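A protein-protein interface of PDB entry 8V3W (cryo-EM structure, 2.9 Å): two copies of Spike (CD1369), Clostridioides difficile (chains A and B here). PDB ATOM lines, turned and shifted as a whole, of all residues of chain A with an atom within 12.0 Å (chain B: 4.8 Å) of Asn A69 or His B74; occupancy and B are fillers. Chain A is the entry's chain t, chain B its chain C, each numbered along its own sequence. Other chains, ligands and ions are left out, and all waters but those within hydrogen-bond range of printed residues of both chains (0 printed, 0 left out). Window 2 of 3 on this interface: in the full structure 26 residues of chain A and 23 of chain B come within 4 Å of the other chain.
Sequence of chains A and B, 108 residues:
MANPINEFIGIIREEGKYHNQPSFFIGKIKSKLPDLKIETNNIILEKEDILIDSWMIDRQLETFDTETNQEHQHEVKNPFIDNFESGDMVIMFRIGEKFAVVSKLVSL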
ATOM      1  N   PHE A  64     -22.767  19.528   7.611  1.00  0.00           N
ATOM      2  CA  PHE A  64     -22.225  18.800   8.749  1.00  0.00           C
ATOM      3  C   PHE A  64     -21.584  17.515   8.242  1.00  0.00           C
ATOM      4  O   PHE A  64     -21.804  17.102   7.100  1.00  0.00           O
ATOM      5  CB  PHE A  64     -23.297  18.524   9.815  1.00  0.00           C
ATOM      6  CG  PHE A  64     -24.482  17.739   9.318  1.00  0.00           C
ATOM      7  CD1 PHE A  64     -25.483  18.352   8.585  1.00  0.00           C
ATOM      8  CD2 PHE A  64     -24.621  16.399   9.635  1.00  0.00           C
ATOM      9  CE1 PHE A  64     -26.582  17.633   8.145  1.00  0.00           C
ATOM     10  CE2 PHE A  64     -25.720  15.678   9.205  1.00  0.00           C
ATOM     11  CZ  PHE A  64     -26.698  16.295   8.457  1.00  0.00           C
ATOM     12  N   ASP A  65     -20.766  16.897   9.094  1.00  0.00           N
ATOM     13  CA  ASP A  65     -19.914  15.781   8.707  1.00  0.00           C
ATOM     14  C   ASP A  65     -20.237  14.538   9.524  1.00  0.00           C
ATOM     15  O   ASP A  65     -20.764  14.625  10.637  1.00  0.00           O
ATOM     16  CB  ASP A  65     -18.434  16.129   8.887  1.00  0.00           C
ATOM     17  CG  ASP A  65     -17.918  17.059   7.813  1.00  0.00           C
ATOM     18  OD1 ASP A  65     -18.616  17.224   6.789  1.00  0.00           O
ATOM     19  OD2 ASP A  65     -16.819  17.623   7.990  1.00  0.00           O
ATOM     20  N   THR A  66     -19.913  13.378   8.961  1.00  0.00           N
ATOM     21  CA  THR A  66     -20.088  12.102   9.637  1.00  0.00           C
ATOM     22  C   THR A  66     -18.787  11.668  10.310  1.00  0.00           C
ATOM     23  O   THR A  66     -17.726  12.264  10.113  1.00  0.00           O
ATOM     24  CB  THR A  66     -20.555  11.031   8.653  1.00  0.00           C
ATOM     25  OG1 THR A  66     -20.688   9.782   9.340  1.00  0.00           O
ATOM     26  CG2 THR A  66     -19.548  10.869   7.533  1.00  0.00           C
ATOM     27  N   GLU A  67     -18.877  10.612  11.118  1.00  0.00           N
ATOM     28  CA  GLU A  67     -17.690  10.059  11.753  1.00  0.00           C
ATOM     29  C   GLU A  67     -16.814   9.352  10.729  1.00  0.00           C
ATOM     30  O   GLU A  67     -17.250   8.998   9.631  1.00  0.00           O
ATOM     31  CB  GLU A  67     -18.053   9.059  12.849  1.00  0.00           C
ATOM     32  CG  GLU A  67     -18.644   9.655  14.100  1.00  0.00           C
ATOM     33  CD  GLU A  67     -17.597  10.237  15.008  1.00  0.00           C
ATOM     34  OE1 GLU A  67     -16.458   9.728  15.012  1.00  0.00           O
ATOM     35  OE2 GLU A  67     -17.914  11.199  15.728  1.00  0.00           O
ATOM     36  N   THR A  68     -15.562   9.138  11.110  1.00  0.00           N
ATOM     37  CA  THR A  68     -14.636   8.424  10.253  1.00  0.00           C
ATOM     38  C   THR A  68     -14.834   6.917  10.388  1.00  0.00           C
ATOM     39  O   THR A  68     -15.195   6.401  11.449  1.00  0.00           O
ATOM     40  CB  THR A  68     -13.190   8.812  10.577  1.00  0.00           C
ATOM     41  OG1 THR A  68     -12.374   8.624   9.414  1.00  0.00           O
ATOM     42  CG2 THR A  68     -12.631   7.973  11.718  1.00  0.00           C
ATOM     43  N   ASN A  69     -14.635   6.221   9.272  1.00  0.00           N
ATOM     44  CA  ASN A  69     -14.662   4.769   9.208  1.00  0.00           C
ATOM     45  C   ASN A  69     -14.028   4.358   7.894  1.00  0.00           C
ATOM     46  O   ASN A  69     -14.186   5.052   6.886  1.00  0.00           O
ATOM     47  CB  ASN A  69     -16.087   4.214   9.308  1.00  0.00           C
ATOM     48  CG  ASN A  69     -16.112   2.707   9.487  1.00  0.00           C
ATOM     49  OD1 ASN A  69     -15.158   2.115   9.988  1.00  0.00           O
ATOM     50  ND2 ASN A  69     -17.206   2.080   9.074  1.00  0.00           N
ATOM     51  N   GLN A  70     -13.308   3.235   7.913  1.00  0.00           N
ATOM     52  CA  GLN A  70     -12.552   2.764   6.752  1.00  0.00           C
ATOM     53  C   GLN A  70     -11.589   3.834   6.249  1.00  0.00           C
ATOM     54  O   GLN A  70     -11.346   3.949   5.044  1.00  0.00           O
ATOM     55  CB  GLN A  70     -13.484   2.307   5.627  1.00  0.00           C
ATOM     56  CG  GLN A  70     -14.083   0.935   5.847  1.00  0.00           C
ATOM     57  CD  GLN A  70     -13.089  -0.176   5.607  1.00  0.00           C
ATOM     58  OE1 GLN A  70     -12.606  -0.363   4.493  1.00  0.00           O
ATOM     59  NE2 GLN A  70     -12.766  -0.916   6.660  1.00  0.00           N
ATOM     60  N   GLU A  71     -11.053   4.629   7.177  1.00  0.00           N
ATOM     61  CA  GLU A  71     -10.041   5.645   6.882  1.00  0.00           C
ATOM     62  C   GLU A  71     -10.532   6.657   5.849  1.00  0.00           C
ATOM     63  O   GLU A  71      -9.768   7.126   5.003  1.00  0.00           O
ATOM     64  CB  GLU A  71      -8.732   4.998   6.432  1.00  0.00           C
ATOM     65  CG  GLU A  71      -8.165   4.012   7.437  1.00  0.00           C
ATOM     66  CD  GLU A  71      -8.714   2.613   7.248  1.00  0.00           C
ATOM     67  OE1 GLU A  71      -8.790   2.156   6.087  1.00  0.00           O
ATOM     68  OE2 GLU A  71      -9.080   1.975   8.256  1.00  0.00           O
ATOM     69  N   HIS A  72     -11.815   7.001   5.920  1.00  0.00           N
ATOM     70  CA  HIS A  72     -12.378   8.022   5.051  1.00  0.00           C
ATOM     71  C   HIS A  72     -13.634   8.589   5.694  1.00  0.00           C
ATOM     72  O   HIS A  72     -14.261   7.956   6.549  1.00  0.00           O
ATOM     73  CB  HIS A  72     -12.676   7.469   3.652  1.00  0.00           C
ATOM     74  CG  HIS A  72     -13.904   6.619   3.586  1.00  0.00           C
ATOM     75  ND1 HIS A  72     -13.876   5.260   3.814  1.00  0.00           N
ATOM     76  CD2 HIS A  72     -15.192   6.928   3.310  1.00  0.00           C
ATOM     77  CE1 HIS A  72     -15.096   4.771   3.685  1.00  0.00           C
ATOM     78  NE2 HIS A  72     -15.913   5.763   3.383  1.00  0.00           N
ATOM     79  N   GLN A  73     -13.993   9.798   5.273  1.00  0.00           N
ATOM     80  CA  GLN A  73     -15.152  10.508   5.795  1.00  0.00           C
ATOM     81  C   GLN A  73     -16.011  10.997   4.639  1.00  0.00           C
ATOM     82  O   GLN A  73     -15.601  10.990   3.477  1.00  0.00           O
ATOM     83  CB  GLN A  73     -14.747  11.698   6.670  1.00  0.00           C
ATOM     84  CG  GLN A  73     -14.337  11.340   8.079  1.00  0.00           C
ATOM     85  CD  GLN A  73     -14.377  12.538   9.003  1.00  0.00           C
ATOM     86  OE1 GLN A  73     -15.116  13.492   8.764  1.00  0.00           O
ATOM     87  NE2 GLN A  73     -13.581  12.500  10.062  1.00  0.00           N
ATOM     88  N   HIS A  74     -17.222  11.421   4.977  1.00  0.00           N
ATOM     89  CA  HIS A  74     -18.139  12.003   4.013  1.00  0.00           C
ATOM     90  C   HIS A  74     -18.695  13.310   4.555  1.00  0.00           C
ATOM     91  O   HIS A  74     -18.762  13.528   5.767  1.00  0.00           O
ATOM     92  CB  HIS A  74     -19.289  11.050   3.670  1.00  0.00           C
ATOM     93  CG  HIS A  74     -18.842   9.748   3.082  1.00  0.00           C
ATOM     94  ND1 HIS A  74     -18.562   9.597   1.741  1.00  0.00           N
ATOM     95  CD2 HIS A  74     -18.628   8.539   3.649  1.00  0.00           C
ATOM     96  CE1 HIS A  74     -18.197   8.350   1.508  1.00  0.00           C
ATOM     97  NE2 HIS A  74     -18.226   7.688   2.650  1.00  0.00           N
ATOM     98  N   GLU A  75     -19.086  14.178   3.633  1.00  0.00           N
ATOM     99  CA  GLU A  75     -19.716  15.455   3.933  1.00  0.00           C
ATOM    100  C   GLU A  75     -21.169  15.364   3.494  1.00  0.00           C
ATOM    101  O   GLU A  75     -21.446  14.995   2.353  1.00  0.00           O
ATOM    102  CB  GLU A  75     -18.998  16.588   3.205  1.00  0.00           C
ATOM    103  CG  GLU A  75     -19.833  17.828   2.989  1.00  0.00           C
ATOM    104  CD  GLU A  75     -19.004  19.095   2.991  1.00  0.00           C
ATOM    105  OE1 GLU A  75     -18.756  19.642   1.896  1.00  0.00           O
ATOM    106  OE2 GLU A  75     -18.602  19.546   4.084  1.00  0.00           O
ATOM    107  N   VAL A  76     -22.096  15.663   4.395  1.00  0.00           N
ATOM    108  CA  VAL A  76     -23.521  15.581   4.095  1.00  0.00           C
ATOM    109  C   VAL A  76     -24.128  16.976   4.176  1.00  0.00           C
ATOM    110  O   VAL A  76     -23.943  17.687   5.172  1.00  0.00           O
ATOM    111  CB  VAL A  76     -24.234  14.585   5.027  1.00  0.00           C
ATOM    112  CG1 VAL A  76     -23.904  14.875   6.467  1.00  0.00           C
ATOM    113  CG2 VAL A  76     -25.735  14.618   4.801  1.00  0.00           C
ATOM    114  N   ASP B  65     -27.325   6.311  12.304  1.00  0.00           N
ATOM    115  CA  ASP B  65     -26.438   5.623  11.376  1.00  0.00           C
ATOM    116  C   ASP B  65     -26.954   5.722   9.946  1.00  0.00           C
ATOM    117  O   ASP B  65     -28.149   5.920   9.712  1.00  0.00           O
ATOM    118  CB  ASP B  65     -26.287   4.147  11.754  1.00  0.00           C
ATOM    119  CG  ASP B  65     -25.319   3.936  12.898  1.00  0.00           C
ATOM    120  OD1 ASP B  65     -24.504   4.846  13.160  1.00  0.00           O
ATOM    121  OD2 ASP B  65     -25.370   2.859  13.528  1.00  0.00           O
ATOM    122  N   THR B  66     -26.039   5.583   8.990  1.00  0.00           N
ATOM    123  CA  THR B  66     -26.378   5.586   7.575  1.00  0.00           C
ATOM    124  C   THR B  66     -26.525   4.156   7.053  1.00  0.00           C
ATOM    125  O   THR B  66     -26.200   3.181   7.733  1.00  0.00           O
ATOM    126  CB  THR B  66     -25.316   6.334   6.771  1.00  0.00           C
ATOM    127  OG1 THR B  66     -25.656   6.294   5.381  1.00  0.00           O
ATOM    128  CG2 THR B  66     -23.958   5.690   6.961  1.00  0.00           C
ATOM    129  N   HIS B  72     -19.311  -1.207   4.086  1.00  0.00           N
ATOM    130  CA  HIS B  72     -18.932  -0.439   5.262  1.00  0.00           C
ATOM    131  C   HIS B  72     -20.020   0.578   5.569  1.00  0.00           C
ATOM    132  O   HIS B  72     -20.807   0.960   4.700  1.00  0.00           O
ATOM    133  CB  HIS B  72     -17.575   0.249   5.069  1.00  0.00           C
ATOM    134  CG  HIS B  72     -17.629   1.459   4.193  1.00  0.00           C
ATOM    135  ND1 HIS B  72     -17.474   1.390   2.826  1.00  0.00           N
ATOM    136  CD2 HIS B  72     -17.812   2.767   4.487  1.00  0.00           C
ATOM    137  CE1 HIS B  72     -17.565   2.603   2.314  1.00  0.00           C
ATOM    138  NE2 HIS B  72     -17.771   3.457   3.300  1.00  0.00           N
ATOM    139  N   GLN B  73     -20.054   1.012   6.826  1.00  0.00           N
ATOM    140  CA  GLN B  73     -21.043   1.961   7.312  1.00  0.00           C
ATOM    141  C   GLN B  73     -20.342   3.100   8.036  1.00  0.00           C
ATOM    142  O   GLN B  73     -19.159   3.021   8.376  1.00  0.00           O
ATOM    143  CB  GLN B  73     -22.051   1.301   8.261  1.00  0.00           C
ATOM    144  CG  GLN B  73     -23.148   0.512   7.584  1.00  0.00           C
ATOM    145  CD  GLN B  73     -24.322   0.271   8.509  1.00  0.00           C
ATOM    146  OE1 GLN B  73     -24.552   1.031   9.448  1.00  0.00           O
ATOM    147  NE2 GLN B  73     -25.070  -0.795   8.254  1.00  0.00           N
ATOM    148  N   HIS B  74     -21.092   4.168   8.269  1.00  0.00           N
ATOM    149  CA  HIS B  74     -20.607   5.308   9.028  1.00  0.00           C
ATOM    150  C   HIS B  74     -21.607   5.667  10.114  1.00  0.00           C
ATOM    151  O   HIS B  74     -22.800   5.374  10.014  1.00  0.00           O
ATOM    152  CB  HIS B  74     -20.352   6.525   8.133  1.00  0.00           C
ATOM    153  CG  HIS B  74     -19.340   6.286   7.059  1.00  0.00           C
ATOM    154  ND1 HIS B  74     -17.984   6.395   7.279  1.00  0.00           N
ATOM    155  CD2 HIS B  74     -19.482   5.942   5.758  1.00  0.00           C
ATOM    156  CE1 HIS B  74     -17.335   6.132   6.159  1.00  0.00           C
ATOM    157  NE2 HIS B  74     -18.222   5.854   5.222  1.00  0.00           N
ATOM    158  N   GLU B  75     -21.092   6.296  11.160  1.00  0.00           N
ATOM    159  CA  GLU B  75     -21.883   6.802  12.271  1.00  0.00           C
ATOM    160  C   GLU B  75     -21.856   8.320  12.186  1.00  0.00           C
ATOM    161  O   GLU B  75     -20.797   8.906  11.965  1.00  0.00           O
ATOM    162  CB  GLU B  75     -21.313   6.307  13.601  1.00  0.00           C
ATOM    163  CG  GLU B  75     -21.992   6.861  14.826  1.00  0.00           C
ATOM    164  CD  GLU B  75     -21.636   6.100  16.089  1.00  0.00           C
ATOM    165  OE1 GLU B  75     -20.539   6.331  16.641  1.00  0.00           O
ATOM    166  OE2 GLU B  75     -22.455   5.267  16.534  1.00  0.00           O
ATOM    167  N   VAL B  76     -23.014   8.956  12.281  1.00  0.00           N
ATOM    168  CA  VAL B  76     -23.101  10.411  12.211  1.00  0.00           C
ATOM    169  C   VAL B  76     -23.687  10.937  13.514  1.00  0.00           C
ATOM    170  O   VAL B  76     -24.731  10.456  13.973  1.00  0.00           O
ATOM    171  CB  VAL B  76     -23.913  10.863  10.983  1.00  0.00           C
ATOM    172  CG1 VAL B  76     -25.236  10.144  10.923  1.00  0.00           C
ATOM    173  CG2 VAL B  76     -24.117  12.368  10.997  1.00  0.00           C
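A ring nitrogen (NE2) of His B72 sits at hydrogen-bond distance from a ring nitrogen (NE2) of His A72 (3.0 Å). A ring nitrogen (NE2) of His B74 is in hydrogen-bond range of a ring nitrogen (NE2) of His A72, 3.0 Å away. NE2 of His B74 sits close to NE2 of His A74 (3.2 Å). The backbone carbonyl oxygen of Glu B75 lies within hydrogen-bond range of the side-chain hydroxyl of Thr A66, 2.8 Å away. O of Glu B75 sits at hydrogen-bond distance from N of Glu A67, at 2.7 Å. ND2 of Asn A69 lies close to O of Gln B73 (2.3 Å).
Printed residues of chain B within 4 Å of Glu A67: His B74 (3.6 Å) and Glu B75 (2.7 Å). Of chain B, only Gln B73 (2.3 Å) and His B74 (3.4 Å) come within 4 Å of Asn A69. Of the printed residues of chain B, Gln A70 touches His B72. Asp B65 touches none of the printed residues of chain A. No residue of chain A comes within 4 Å of Thr B66. Gln B73 touches just one residue of chain A: Asn A69. His B74 touches just these residues of chain A: Thr A66, Glu A67, Asn A69, His A72 and His A74. Glu B75 touches two residues of chain A. Of chain A, only Thr A66 comes within 4 Å of Val B76. The nearest printed residue of chain B that does not touch His A72 is Gln B73 (6.4 Å).
Of the 7 printed residues of chain B, 5 touch a printed residue of chain A. Hydrophobic or aromatic side chains of chain B within 4 Å of the printed part of chain A: His B72, His B74 and Val B76. Printed residues of chain A that touch a printed residue of chain B: Thr A66, Glu A67, Asn A69, Gln A70, His A72 and His A74. Hydrophobic or aromatic side chains of chain A that line the printed part of chain B: His A72 and His A74.
Thr A66 touches His B74. OG1 of Thr A66 touches CB of Val B76, 3.8 Å away. Glu A67 touches His B74 (O to ND1, 3.6 Å). Asn A69 touches His B74. Gln A70 touches His B72 (CG to CB, 3.6 Å).
O of Thr B66 lies close to OE1 of Gln B73 (3.2 Å). The backbone NH of Thr B66 lies close to the backbone carbonyl oxygen of His B74 (3.4 Å). The side-chain amide oxygen (OE1) of Gln A73 lies close to the backbone carbonyl oxygen (O) of Thr A66 (3.2 Å). ND1 of His A72 sits at hydrogen-bond distance from O of Asn A69 (3.1 Å). A ring nitrogen (ND1) of His A72 sits at hydrogen-bond distance from the backbone carbonyl oxygen (O) of Gln A70, at 3.1 Å. A ring nitrogen (NE2) of His A72 sits at hydrogen-bond distance from a ring nitrogen (NE2) of His A74.
Thr A66 touches His B74, but with the chains exchanged His A74 does not touch Thr B66 (6.9 Å). Thr A66 touches Glu B75, but with the chains exchanged Glu A75 does not touch Thr B66 (10.1 Å). His A72 touches its own counterpart, His B72. His B74 touches its own counterpart, His A74. Positions printed for both chains: 65, 66, 72, 73, 74, 75 and 76. Of the 11 pairs that touch across the chains among the printed residues, 2 have their exchanged pair printed and touching as well.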
